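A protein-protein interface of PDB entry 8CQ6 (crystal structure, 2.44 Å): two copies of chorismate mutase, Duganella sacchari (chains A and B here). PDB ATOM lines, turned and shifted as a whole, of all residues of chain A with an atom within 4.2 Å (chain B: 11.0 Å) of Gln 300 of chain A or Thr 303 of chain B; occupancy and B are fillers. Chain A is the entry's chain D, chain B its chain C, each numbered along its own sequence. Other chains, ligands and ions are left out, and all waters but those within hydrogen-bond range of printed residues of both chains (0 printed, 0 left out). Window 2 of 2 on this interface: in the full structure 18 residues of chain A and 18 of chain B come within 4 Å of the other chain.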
ATOM      1  N   ALA A 296      -5.738  32.142 -29.450  1.00  0.00           N
ATOM      2  CA  ALA A 296      -4.805  31.029 -29.331  1.00  0.00           C
ATOM      3  C   ALA A 296      -4.718  30.528 -27.887  1.00  0.00           C
ATOM      4  O   ALA A 296      -4.599  29.326 -27.650  1.00  0.00           O
ATOM      5  CB  ALA A 296      -3.448  31.444 -29.840  1.00  0.00           C
ATOM      6  N   ALA A 297      -4.767  31.450 -26.918  1.00  0.00           N
ATOM      7  CA  ALA A 297      -4.757  31.068 -25.517  1.00  0.00           C
ATOM      8  C   ALA A 297      -6.004  30.253 -25.179  1.00  0.00           C
ATOM      9  O   ALA A 297      -5.917  29.252 -24.478  1.00  0.00           O
ATOM     10  CB  ALA A 297      -4.652  32.291 -24.643  1.00  0.00           C
ATOM     11  N   VAL A 298      -7.165  30.694 -25.671  1.00  0.00           N
ATOM     12  CA  VAL A 298      -8.422  30.033 -25.359  1.00  0.00           C
ATOM     13  C   VAL A 298      -8.393  28.611 -25.913  1.00  0.00           C
ATOM     14  O   VAL A 298      -8.790  27.674 -25.229  1.00  0.00           O
ATOM     15  CB  VAL A 298      -9.627  30.820 -25.903  1.00  0.00           C
ATOM     16  CG1 VAL A 298     -10.896  29.981 -25.913  1.00  0.00           C
ATOM     17  CG2 VAL A 298      -9.856  32.096 -25.109  1.00  0.00           C
ATOM     18  N   GLN A 299      -7.933  28.465 -27.156  1.00  0.00           N
ATOM     19  CA  GLN A 299      -7.855  27.163 -27.797  1.00  0.00           C
ATOM     20  C   GLN A 299      -6.999  26.216 -26.957  1.00  0.00           C
ATOM     21  O   GLN A 299      -7.439  25.123 -26.618  1.00  0.00           O
ATOM     22  CB  GLN A 299      -7.253  27.281 -29.202  1.00  0.00           C
ATOM     23  CG  GLN A 299      -8.263  27.316 -30.332  1.00  0.00           C
ATOM     24  CD  GLN A 299      -7.757  26.541 -31.530  1.00  0.00           C
ATOM     25  OE1 GLN A 299      -6.659  25.983 -31.511  1.00  0.00           O
ATOM     26  NE2 GLN A 299      -8.561  26.492 -32.580  1.00  0.00           N
ATOM     27  N   GLN A 300      -5.772  26.654 -26.649  1.00  0.00           N
ATOM     28  CA  GLN A 300      -4.828  25.880 -25.856  1.00  0.00           C
ATOM     29  C   GLN A 300      -5.428  25.551 -24.487  1.00  0.00           C
ATOM     30  O   GLN A 300      -5.220  24.463 -23.962  1.00  0.00           O
ATOM     31  CB  GLN A 300      -3.543  26.676 -25.619  1.00  0.00           C
ATOM     32  CG  GLN A 300      -2.435  26.480 -26.637  1.00  0.00           C
ATOM     33  CD  GLN A 300      -1.172  27.156 -26.162  1.00  0.00           C
ATOM     34  OE1 GLN A 300      -0.389  26.628 -25.368  1.00  0.00           O
ATOM     35  NE2 GLN A 300      -0.960  28.364 -26.650  1.00  0.00           N
ATOM     36  N   GLY A 301      -6.153  26.516 -23.914  1.00  0.00           N
ATOM     37  CA  GLY A 301      -6.781  26.355 -22.617  1.00  0.00           C
ATOM     38  C   GLY A 301      -7.885  25.305 -22.617  1.00  0.00           C
ATOM     39  O   GLY A 301      -8.084  24.631 -21.606  1.00  0.00           O
ATOM     40  N   ARG A 302      -8.593  25.171 -23.746  1.00  0.00           N
ATOM     41  CA  ARG A 302      -9.647  24.177 -23.863  1.00  0.00           C
ATOM     42  C   ARG A 302      -9.060  22.770 -23.793  1.00  0.00           C
ATOM     43  O   ARG A 302      -9.669  21.877 -23.208  1.00  0.00           O
ATOM     44  CB  ARG A 302     -10.417  24.348 -25.171  1.00  0.00           C
ATOM     45  CG  ARG A 302     -11.313  25.572 -25.187  1.00  0.00           C
ATOM     46  CD  ARG A 302     -12.758  25.223 -25.491  1.00  0.00           C
ATOM     47  NE  ARG A 302     -13.562  26.426 -25.670  1.00  0.00           N
ATOM     48  CZ  ARG A 302     -13.396  27.310 -26.651  1.00  0.00           C
ATOM     49  NH1 ARG A 302     -12.688  26.989 -27.721  1.00  0.00           N
ATOM     50  NH2 ARG A 302     -13.943  28.510 -26.561  1.00  0.00           N
ATOM     51  N   THR A 303      -7.865  22.592 -24.368  1.00  0.00           N
ATOM     52  CA  THR A 303      -7.209  21.295 -24.355  1.00  0.00           C
ATOM     53  C   THR A 303      -6.774  20.941 -22.930  1.00  0.00           C
ATOM     54  O   THR A 303      -6.702  19.761 -22.586  1.00  0.00           O
ATOM     55  CB  THR A 303      -6.053  21.236 -25.362  1.00  0.00           C
ATOM     56  OG1 THR A 303      -4.914  21.886 -24.799  1.00  0.00           O
ATOM     57  CG2 THR A 303      -6.400  21.872 -26.688  1.00  0.00           C
ATOM     58  N   LEU A 304      -6.511  21.961 -22.097  1.00  0.00           N
ATOM     59  CA  LEU A 304      -6.152  21.748 -20.702  1.00  0.00           C
ATOM     60  C   LEU A 304      -7.388  21.762 -19.805  1.00  0.00           C
ATOM     61  O   LEU A 304      -7.257  21.658 -18.589  1.00  0.00           O
ATOM     62  CB  LEU A 304      -5.168  22.834 -20.258  1.00  0.00           C
ATOM     63  CG  LEU A 304      -3.782  22.775 -20.892  1.00  0.00           C
ATOM     64  CD1 LEU A 304      -3.085  24.125 -20.811  1.00  0.00           C
ATOM     65  CD2 LEU A 304      -2.941  21.708 -20.226  1.00  0.00           C
ATOM     66  N   THR A 360       2.039  29.374 -23.167  1.00  0.00           N
ATOM     67  CA  THR A 360       1.945  27.954 -22.883  1.00  0.00           C
ATOM     68  C   THR A 360       2.241  27.704 -21.400  1.00  0.00           C
ATOM     69  O   THR A 360       1.420  27.138 -20.664  1.00  0.00           O
ATOM     70  CB  THR A 360       2.895  27.160 -23.789  1.00  0.00           C
ATOM     71  OG1 THR A 360       2.637  27.466 -25.161  1.00  0.00           O
ATOM     72  CG2 THR A 360       2.769  25.664 -23.577  1.00  0.00           C
ATOM     73  N   LEU A 363      -0.467  29.021 -19.042  1.00  0.00           N
ATOM     74  CA  LEU A 363      -1.708  28.262 -19.077  1.00  0.00           C
ATOM     75  C   LEU A 363      -1.579  26.961 -18.278  1.00  0.00           C
ATOM     76  O   LEU A 363      -2.513  26.561 -17.582  1.00  0.00           O
ATOM     77  CB  LEU A 363      -2.064  27.960 -20.537  1.00  0.00           C
ATOM     78  CG  LEU A 363      -2.607  29.137 -21.340  1.00  0.00           C
ATOM     79  CD1 LEU A 363      -2.491  28.886 -22.829  1.00  0.00           C
ATOM     80  CD2 LEU A 363      -4.046  29.425 -20.955  1.00  0.00           C
ATOM     81  N   ARG A 364      -0.430  26.287 -18.403  1.00  0.00           N
ATOM     82  CA  ARG A 364      -0.221  25.018 -17.724  1.00  0.00           C
ATOM     83  C   ARG A 364      -0.193  25.227 -16.210  1.00  0.00           C
ATOM     84  O   ARG A 364      -0.715  24.410 -15.448  1.00  0.00           O
ATOM     85  CB  ARG A 364       1.094  24.378 -18.169  1.00  0.00           C
ATOM     86  CG  ARG A 364       1.034  23.653 -19.502  1.00  0.00           C
ATOM     87  CD  ARG A 364       2.211  22.705 -19.651  1.00  0.00           C
ATOM     88  NE  ARG A 364       3.341  23.318 -20.344  1.00  0.00           N
ATOM     89  CZ  ARG A 364       3.853  22.881 -21.484  1.00  0.00           C
ATOM     90  NH1 ARG A 364       3.102  22.192 -22.323  1.00  0.00           N
ATOM     91  NH2 ARG A 364       5.112  23.150 -21.781  1.00  0.00           N
ATOM     92  N   ALA B 295      -0.624  16.202 -37.095  1.00  0.00           N
ATOM     93  CA  ALA B 295      -0.019  17.498 -36.833  1.00  0.00           C
ATOM     94  C   ALA B 295      -0.759  18.190 -35.697  1.00  0.00           C
ATOM     95  O   ALA B 295      -0.121  18.774 -34.827  1.00  0.00           O
ATOM     96  CB  ALA B 295      -0.027  18.356 -38.077  1.00  0.00           C
ATOM     97  N   ALA B 296      -2.097  18.095 -35.718  1.00  0.00           N
ATOM     98  CA  ALA B 296      -2.957  18.720 -34.722  1.00  0.00           C
ATOM     99  C   ALA B 296      -2.844  18.006 -33.373  1.00  0.00           C
ATOM    100  O   ALA B 296      -2.881  18.650 -32.334  1.00  0.00           O
ATOM    101  CB  ALA B 296      -4.384  18.733 -35.216  1.00  0.00           C
ATOM    102  N   ALA B 297      -2.715  16.677 -33.387  1.00  0.00           N
ATOM    103  CA  ALA B 297      -2.525  15.920 -32.161  1.00  0.00           C
ATOM    104  C   ALA B 297      -1.211  16.313 -31.491  1.00  0.00           C
ATOM    105  O   ALA B 297      -1.160  16.481 -30.281  1.00  0.00           O
ATOM    106  CB  ALA B 297      -2.570  14.444 -32.453  1.00  0.00           C
ATOM    107  N   VAL B 298      -0.144  16.444 -32.279  1.00  0.00           N
ATOM    108  CA  VAL B 298       1.170  16.751 -31.739  1.00  0.00           C
ATOM    109  C   VAL B 298       1.128  18.129 -31.087  1.00  0.00           C
ATOM    110  O   VAL B 298       1.651  18.307 -29.990  1.00  0.00           O
ATOM    111  CB  VAL B 298       2.257  16.681 -32.828  1.00  0.00           C
ATOM    112  CG1 VAL B 298       3.542  17.350 -32.388  1.00  0.00           C
ATOM    113  CG2 VAL B 298       2.537  15.248 -33.256  1.00  0.00           C
ATOM    114  N   GLN B 299       0.518  19.097 -31.774  1.00  0.00           N
ATOM    115  CA  GLN B 299       0.416  20.456 -31.264  1.00  0.00           C
ATOM    116  C   GLN B 299      -0.293  20.450 -29.912  1.00  0.00           C
ATOM    117  O   GLN B 299       0.225  20.993 -28.944  1.00  0.00           O
ATOM    118  CB  GLN B 299      -0.339  21.362 -32.243  1.00  0.00           C
ATOM    119  CG  GLN B 299       0.557  22.159 -33.184  1.00  0.00           C
ATOM    120  CD  GLN B 299       1.342  23.247 -32.493  1.00  0.00           C
ATOM    121  OE1 GLN B 299       2.472  23.040 -32.055  1.00  0.00           O
ATOM    122  NE2 GLN B 299       0.746  24.427 -32.402  1.00  0.00           N
ATOM    123  N   GLN B 300      -1.485  19.841 -29.870  1.00  0.00           N
ATOM    124  CA  GLN B 300      -2.292  19.731 -28.660  1.00  0.00           C
ATOM    125  C   GLN B 300      -1.500  19.020 -27.563  1.00  0.00           C
ATOM    126  O   GLN B 300      -1.596  19.373 -26.393  1.00  0.00           O
ATOM    127  CB  GLN B 300      -3.556  18.901 -28.913  1.00  0.00           C
ATOM    128  CG  GLN B 300      -4.793  19.672 -29.332  1.00  0.00           C
ATOM    129  CD  GLN B 300      -5.996  18.760 -29.346  1.00  0.00           C
ATOM    130  OE1 GLN B 300      -6.646  18.500 -28.329  1.00  0.00           O
ATOM    131  NE2 GLN B 300      -6.321  18.263 -30.525  1.00  0.00           N
ATOM    132  N   GLY B 301      -0.742  17.990 -27.953  1.00  0.00           N
ATOM    133  CA  GLY B 301       0.057  17.210 -27.030  1.00  0.00           C
ATOM    134  C   GLY B 301       1.186  18.021 -26.409  1.00  0.00           C
ATOM    135  O   GLY B 301       1.555  17.770 -25.267  1.00  0.00           O
ATOM    136  N   ARG B 302       1.743  18.977 -27.156  1.00  0.00           N
ATOM    137  CA  ARG B 302       2.813  19.819 -26.643  1.00  0.00           C
ATOM    138  C   ARG B 302       2.289  20.697 -25.514  1.00  0.00           C
ATOM    139  O   ARG B 302       3.002  20.933 -24.541  1.00  0.00           O
ATOM    140  CB  ARG B 302       3.405  20.688 -27.751  1.00  0.00           C
ATOM    141  CG  ARG B 302       4.227  19.904 -28.759  1.00  0.00           C
ATOM    142  CD  ARG B 302       5.650  20.406 -28.882  1.00  0.00           C
ATOM    143  NE  ARG B 302       6.340  19.748 -29.981  1.00  0.00           N
ATOM    144  CZ  ARG B 302       6.023  19.882 -31.267  1.00  0.00           C
ATOM    145  NH1 ARG B 302       5.200  20.841 -31.663  1.00  0.00           N
ATOM    146  NH2 ARG B 302       6.525  19.036 -32.153  1.00  0.00           N
ATOM    147  N   THR B 303       1.036  21.145 -25.630  1.00  0.00           N
ATOM    148  CA  THR B 303       0.435  21.979 -24.601  1.00  0.00           C
ATOM    149  C   THR B 303       0.214  21.164 -23.325  1.00  0.00           C
ATOM    150  O   THR B 303       0.232  21.723 -22.227  1.00  0.00           O
ATOM    151  CB  THR B 303      -0.846  22.661 -25.105  1.00  0.00           C
ATOM    152  OG1 THR B 303      -1.923  21.727 -25.054  1.00  0.00           O
ATOM    153  CG2 THR B 303      -0.717  23.197 -26.513  1.00  0.00           C
ATOM    154  N   LEU B 304       0.030  19.843 -23.466  1.00  0.00           N
ATOM    155  CA  LEU B 304      -0.133  18.957 -22.323  1.00  0.00           C
ATOM    156  C   LEU B 304       1.214  18.379 -21.887  1.00  0.00           C
ATOM    157  O   LEU B 304       1.259  17.545 -20.987  1.00  0.00           O
ATOM    158  CB  LEU B 304      -1.093  17.821 -22.691  1.00  0.00           C
ATOM    159  CG  LEU B 304      -2.548  18.220 -22.932  1.00  0.00           C
ATOM    160  CD1 LEU B 304      -3.277  17.161 -23.744  1.00  0.00           C
ATOM    161  CD2 LEU B 304      -3.272  18.479 -21.627  1.00  0.00           C
ATOM    162  N   GLY B 305       2.309  18.783 -22.539  1.00  0.00           N
ATOM    163  CA  GLY B 305       3.648  18.363 -22.149  1.00  0.00           C
ATOM    164  C   GLY B 305       3.969  16.918 -22.537  1.00  0.00           C
ATOM    165  O   GLY B 305       4.986  16.390 -22.097  1.00  0.00           O
ATOM    166  N   LEU B 306       3.115  16.285 -23.356  1.00  0.00           N
ATOM    167  CA  LEU B 306       3.448  15.012 -23.981  1.00  0.00           C
ATOM    168  C   LEU B 306       4.603  15.213 -24.964  1.00  0.00           C
ATOM    169  O   LEU B 306       4.685  16.244 -25.635  1.00  0.00           O
ATOM    170  CB  LEU B 306       2.228  14.455 -24.725  1.00  0.00           C
ATOM    171  CG  LEU B 306       1.121  13.777 -23.917  1.00  0.00           C
ATOM    172  CD1 LEU B 306       1.678  12.864 -22.841  1.00  0.00           C
ATOM    173  CD2 LEU B 306       0.169  14.796 -23.322  1.00  0.00           C
ATOM    174  N   PRO B 307       5.519  14.228 -25.102  1.00  0.00           N
ATOM    175  CA  PRO B 307       6.510  14.246 -26.175  1.00  0.00           C
ATOM    176  C   PRO B 307       5.914  13.845 -27.524  1.00  0.00           C
ATOM    177  O   PRO B 307       5.040  12.988 -27.605  1.00  0.00           O
ATOM    178  CB  PRO B 307       7.554  13.224 -25.695  1.00  0.00           C
ATOM    179  CG  PRO B 307       6.758  12.232 -24.870  1.00  0.00           C
ATOM    180  CD  PRO B 307       5.649  13.046 -24.236  1.00  0.00           C
ATOM    181  N   ASP B 308       6.415  14.481 -28.586  1.00  0.00           N
ATOM    182  CA  ASP B 308       5.738  14.499 -29.871  1.00  0.00           C
ATOM    183  C   ASP B 308       5.914  13.143 -30.551  1.00  0.00           C
ATOM    184  O   ASP B 308       4.971  12.623 -31.143  1.00  0.00           O
ATOM    185  CB  ASP B 308       6.217  15.664 -30.745  1.00  0.00           C
ATOM    186  CG  ASP B 308       7.644  16.117 -30.481  1.00  0.00           C
ATOM    187  OD1 ASP B 308       8.580  15.422 -30.936  1.00  0.00           O
ATOM    188  OD2 ASP B 308       7.808  17.159 -29.801  1.00  0.00           O
ATOM    189  N   VAL B 311       3.184  10.815 -29.263  1.00  0.00           N
ATOM    190  CA  VAL B 311       1.862  11.198 -29.727  1.00  0.00           C
ATOM    191  C   VAL B 311       1.687  10.789 -31.187  1.00  0.00           C
ATOM    192  O   VAL B 311       0.634  10.298 -31.581  1.00  0.00           O
ATOM    193  CB  VAL B 311       1.618  12.705 -29.553  1.00  0.00           C
ATOM    194  CG1 VAL B 311       0.335  13.129 -30.235  1.00  0.00           C
ATOM    195  CG2 VAL B 311       1.588  13.107 -28.093  1.00  0.00           C
ATOM    196  N   THR B 359      -9.964  12.806 -30.081  1.00  0.00           N
ATOM    197  CA  THR B 359      -8.536  13.047 -30.057  1.00  0.00           C
ATOM    198  C   THR B 359      -8.158  13.796 -28.780  1.00  0.00           C
ATOM    199  O   THR B 359      -7.245  13.387 -28.052  1.00  0.00           O
ATOM    200  CB  THR B 359      -8.116  13.784 -31.332  1.00  0.00           C
ATOM    201  OG1 THR B 359      -8.374  12.879 -32.408  1.00  0.00           O
ATOM    202  CG2 THR B 359      -6.663  14.217 -31.335  1.00  0.00           C
ATOM    203  N   THR B 360      -8.883  14.890 -28.517  1.00  0.00           N
ATOM    204  CA  THR B 360      -8.702  15.660 -27.303  1.00  0.00           C
ATOM    205  C   THR B 360      -8.793  14.732 -26.091  1.00  0.00           C
ATOM    206  O   THR B 360      -7.865  14.645 -25.284  1.00  0.00           O
ATOM    207  CB  THR B 360      -9.728  16.795 -27.235  1.00  0.00           C
ATOM    208  OG1 THR B 360      -9.662  17.600 -28.410  1.00  0.00           O
ATOM    209  CG2 THR B 360      -9.490  17.685 -26.033  1.00  0.00           C
ATOM    210  N   LEU B 363      -5.851  12.313 -25.757  1.00  0.00           N
ATOM    211  CA  LEU B 363      -4.600  12.952 -25.370  1.00  0.00           C
ATOM    212  C   LEU B 363      -4.583  13.273 -23.871  1.00  0.00           C
ATOM    213  O   LEU B 363      -3.556  13.109 -23.206  1.00  0.00           O
ATOM    214  CB  LEU B 363      -4.419  14.236 -26.188  1.00  0.00           C
ATOM    215  CG  LEU B 363      -4.017  14.035 -27.647  1.00  0.00           C
ATOM    216  CD1 LEU B 363      -4.307  15.273 -28.476  1.00  0.00           C
ATOM    217  CD2 LEU B 363      -2.550  13.655 -27.765  1.00  0.00           C
ATOM    218  N   ARG B 364      -5.719  13.747 -23.345  1.00  0.00           N
ATOM    219  CA  ARG B 364      -5.803  14.130 -21.944  1.00  0.00           C
ATOM    220  C   ARG B 364      -5.634  12.901 -21.056  1.00  0.00           C
ATOM    221  O   ARG B 364      -4.987  12.967 -20.016  1.00  0.00           O
ATOM    222  CB  ARG B 364      -7.148  14.800 -21.643  1.00  0.00           C
ATOM    223  CG  ARG B 364      -7.219  16.264 -22.041  1.00  0.00           C
ATOM    224  CD  ARG B 364      -8.326  16.998 -21.302  1.00  0.00           C
ATOM    225  NE  ARG B 364      -9.567  17.054 -22.067  1.00  0.00           N
ATOM    226  CZ  ARG B 364     -10.149  18.171 -22.487  1.00  0.00           C
ATOM    227  NH1 ARG B 364      -9.430  19.261 -22.682  1.00  0.00           N
ATOM    228  NH2 ARG B 364     -11.447  18.188 -22.731  1.00  0.00           N
ATOM    229  N   MET B 366      -3.949  10.265 -21.920  1.00  0.00           N
ATOM    230  CA  MET B 366      -2.535   9.926 -22.001  1.00  0.00           C
ATOM    231  C   MET B 366      -1.758  10.778 -21.001  1.00  0.00           C
ATOM    232  O   MET B 366      -0.852  10.281 -20.336  1.00  0.00           O
ATOM    233  CB  MET B 366      -1.962  10.164 -23.404  1.00  0.00           C
ATOM    234  CG  MET B 366      -2.428   9.176 -24.436  1.00  0.00           C
ATOM    235  SD  MET B 366      -2.064   9.719 -26.135  1.00  0.00           S
ATOM    236  CE  MET B 366      -0.279   9.625 -26.154  1.00  0.00           C
ATOM    237  N   ALA B 367      -2.127  12.059 -20.913  1.00  0.00           N
ATOM    238  CA  ALA B 367      -1.367  13.033 -20.147  1.00  0.00           C
ATOM    239  C   ALA B 367      -1.450  12.701 -18.653  1.00  0.00           C
ATOM    240  O   ALA B 367      -0.466  12.822 -17.930  1.00  0.00           O
ATOM    241  CB  ALA B 367      -1.874  14.426 -20.452  1.00  0.00           C
ATOM    242  N   ASP B 368      -2.648  12.320 -18.194  1.00  0.00           N
ATOM    243  CA  ASP B 368      -2.897  12.158 -16.767  1.00  0.00           C
ATOM    244  C   ASP B 368      -2.255  10.857 -16.284  1.00  0.00           C
ATOM    245  O   ASP B 368      -1.633  10.845 -15.221  1.00  0.00           O
ATOM    246  CB  ASP B 368      -4.391  12.270 -16.444  1.00  0.00           C
ATOM    247  CG  ASP B 368      -4.982  13.654 -16.691  1.00  0.00           C
ATOM    248  OD1 ASP B 368      -4.215  14.595 -17.001  1.00  0.00           O
ATOM    249  OD2 ASP B 368      -6.215  13.788 -16.570  1.00  0.00           O
ATOM    250  N   GLN B 370       0.145   8.449 -16.997  1.00  0.00           N
ATOM    251  CA  GLN B 370       1.399   7.989 -17.557  1.00  0.00           C
ATOM    252  C   GLN B 370       1.959   6.881 -16.676  1.00  0.00           C
ATOM    253  O   GLN B 370       2.537   5.933 -17.195  1.00  0.00           O
ATOM    254  CB  GLN B 370       2.400   9.140 -17.652  1.00  0.00           C
ATOM    255  CG  GLN B 370       1.831  10.413 -18.261  1.00  0.00           C
ATOM    256  CD  GLN B 370       2.909  11.351 -18.752  1.00  0.00           C
ATOM    257  OE1 GLN B 370       2.618  12.277 -19.504  1.00  0.00           O
ATOM    258  NE2 GLN B 370       4.141  11.160 -18.300  1.00  0.00           N
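O of Arg 302 of chain B lies within hydrogen-bond range of NH1 of Arg 364 of chain A (2.6 Å). The side-chain hydroxyl (OG1) of Thr 303 of chain B is in hydrogen-bond range of the side-chain hydroxyl (OG1) of Thr 303 of chain A, 3.0 Å away. The backbone carbonyl oxygen of Thr 303 of chain B is in hydrogen-bond range of the guanidinium group of Arg 364 of chain A. The guanidinium group of Arg 364 of chain B lies within hydrogen-bond range of the backbone carbonyl oxygen of Arg 302 of chain A, 2.7 Å away. NH1 of Arg 364 of chain B is in hydrogen-bond range of O of Thr 303 of chain A (2.8 Å).
Gln 300 of chain A touches one residue of chain B. Of chain A, only Gln 300 (3.6 Å), Thr 303 (3.0 Å), Leu 304 (3.8 Å) and Arg 364 (2.9 Å) come within 4 Å of Thr 303 of chain B. No residue of chain B comes within 4 Å of Ala 297 of chain A. Gln 299 of chain A touches none of the printed residues of chain B. No residue of chain B comes within 4 Å of Thr 360 of chain A. Of the printed residues of chain B, Arg 302 of chain A touches Arg 364 (2.7 Å). Of the printed residues of chain A, Leu 304 of chain B touches Thr 303 (3.8 Å) and Leu 304 (3.5 Å). Of the printed residues of chain B, Leu 304 of chain A touches Thr 303 and Leu 304. Ala 297 of chain B touches none of the printed residues of chain A. Leu 306 of chain B touches none of the printed residues of chain A. The nearest printed residue of chain B that does not touch Gln 300 of chain A is Arg 302 of chain B (6.5 Å). The nearest printed residue of chain A that does not touch Thr 303 of chain B is Thr 360 of chain A (4.5 Å). The nearest printed residue of chain A that does not touch Arg 364 of chain B is Leu 304 of chain A (4.02 Å).
Printed residues of chain A that touch a printed residue of chain B: Gln 300, Arg 302, Thr 303, Leu 304 and Arg 364. Hydrophobic or aromatic side chains of chain A within 4 Å of the printed part of chain B: Leu 304. Of the 23 printed residues of chain B, 6 touch a printed residue of chain A. Printed residues of chain B that touch a printed residue of chain A: Gln 300, Arg 302, Thr 303, Leu 304, Gly 305 and Arg 364. Hydrophobic or aromatic side chains of chain B that line the printed part of chain A: Leu 304. Along chain B the printed residues that touch a printed residue of chain A span positions 300 to 364. Among the printed residues, no Asp or Glu carboxylate lies within 4 Å of a Lys or Arg side-chain nitrogen of the other chain.
The backbone carbonyl oxygen (O) of Gln 300 of chain B lies within hydrogen-bond range of the side-chain hydroxyl (OG1) of Thr 303 of chain B, at 2.7 Å. The side-chain hydroxyl (OG1) of Thr 360 of chain B sits at hydrogen-bond distance from the side-chain amide oxygen (OE1) of Gln 300 of chain B, 3.1 Å away. The guanidinium group (NE) of Arg 302 of chain B is in salt-bridge range of the side-chain carboxylate (OD2) of Asp 308 of chain B, at 3.0 Å. OG1 of Thr 303 of chain A lies within hydrogen-bond range of O of Gln 300 of chain A. The side-chain amide oxygen (OE1) of Gln 300 of chain A sits at hydrogen-bond distance from the side-chain hydroxyl (OG1) of Thr 360 of chain A, 3.1 Å away.
Thr 303 of chain B touches its own counterpart, Thr 303 of chain A. Thr 303 of chain A touches Leu 304 of chain B, and with the chains exchanged Leu 304 of chain A touches Thr 303 of chain B. Thr 303 of chain A touches Arg 364 of chain B, and with the chains exchanged Arg 364 of chain A touches Thr 303 of chain B. Leu 304 of chain A touches its own counterpart, Leu 304 of chain B. 12 positions are printed for both chains. Of the 11 pairs that touch across the chains among the printed residues, 10 have their exchanged pair printed and touching as well.
Among the printed residues, merely in contact across the chains: Arg 364 of chain A with Gly 305 of chain B (3.5 Å), Leu 304 of chain A with Leu 304 of chain B (3.5 Å), Gln 300 of chain A with Thr 303 of chain B (3.6 Å), Leu 304 of chain A with Thr 303 of chain B (3.8 Å), Thr 303 of chain A with Gln 300 of chain B (3.8 Å) and Thr 303 of chain A with Leu 304 of chain B (3.8 Å).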
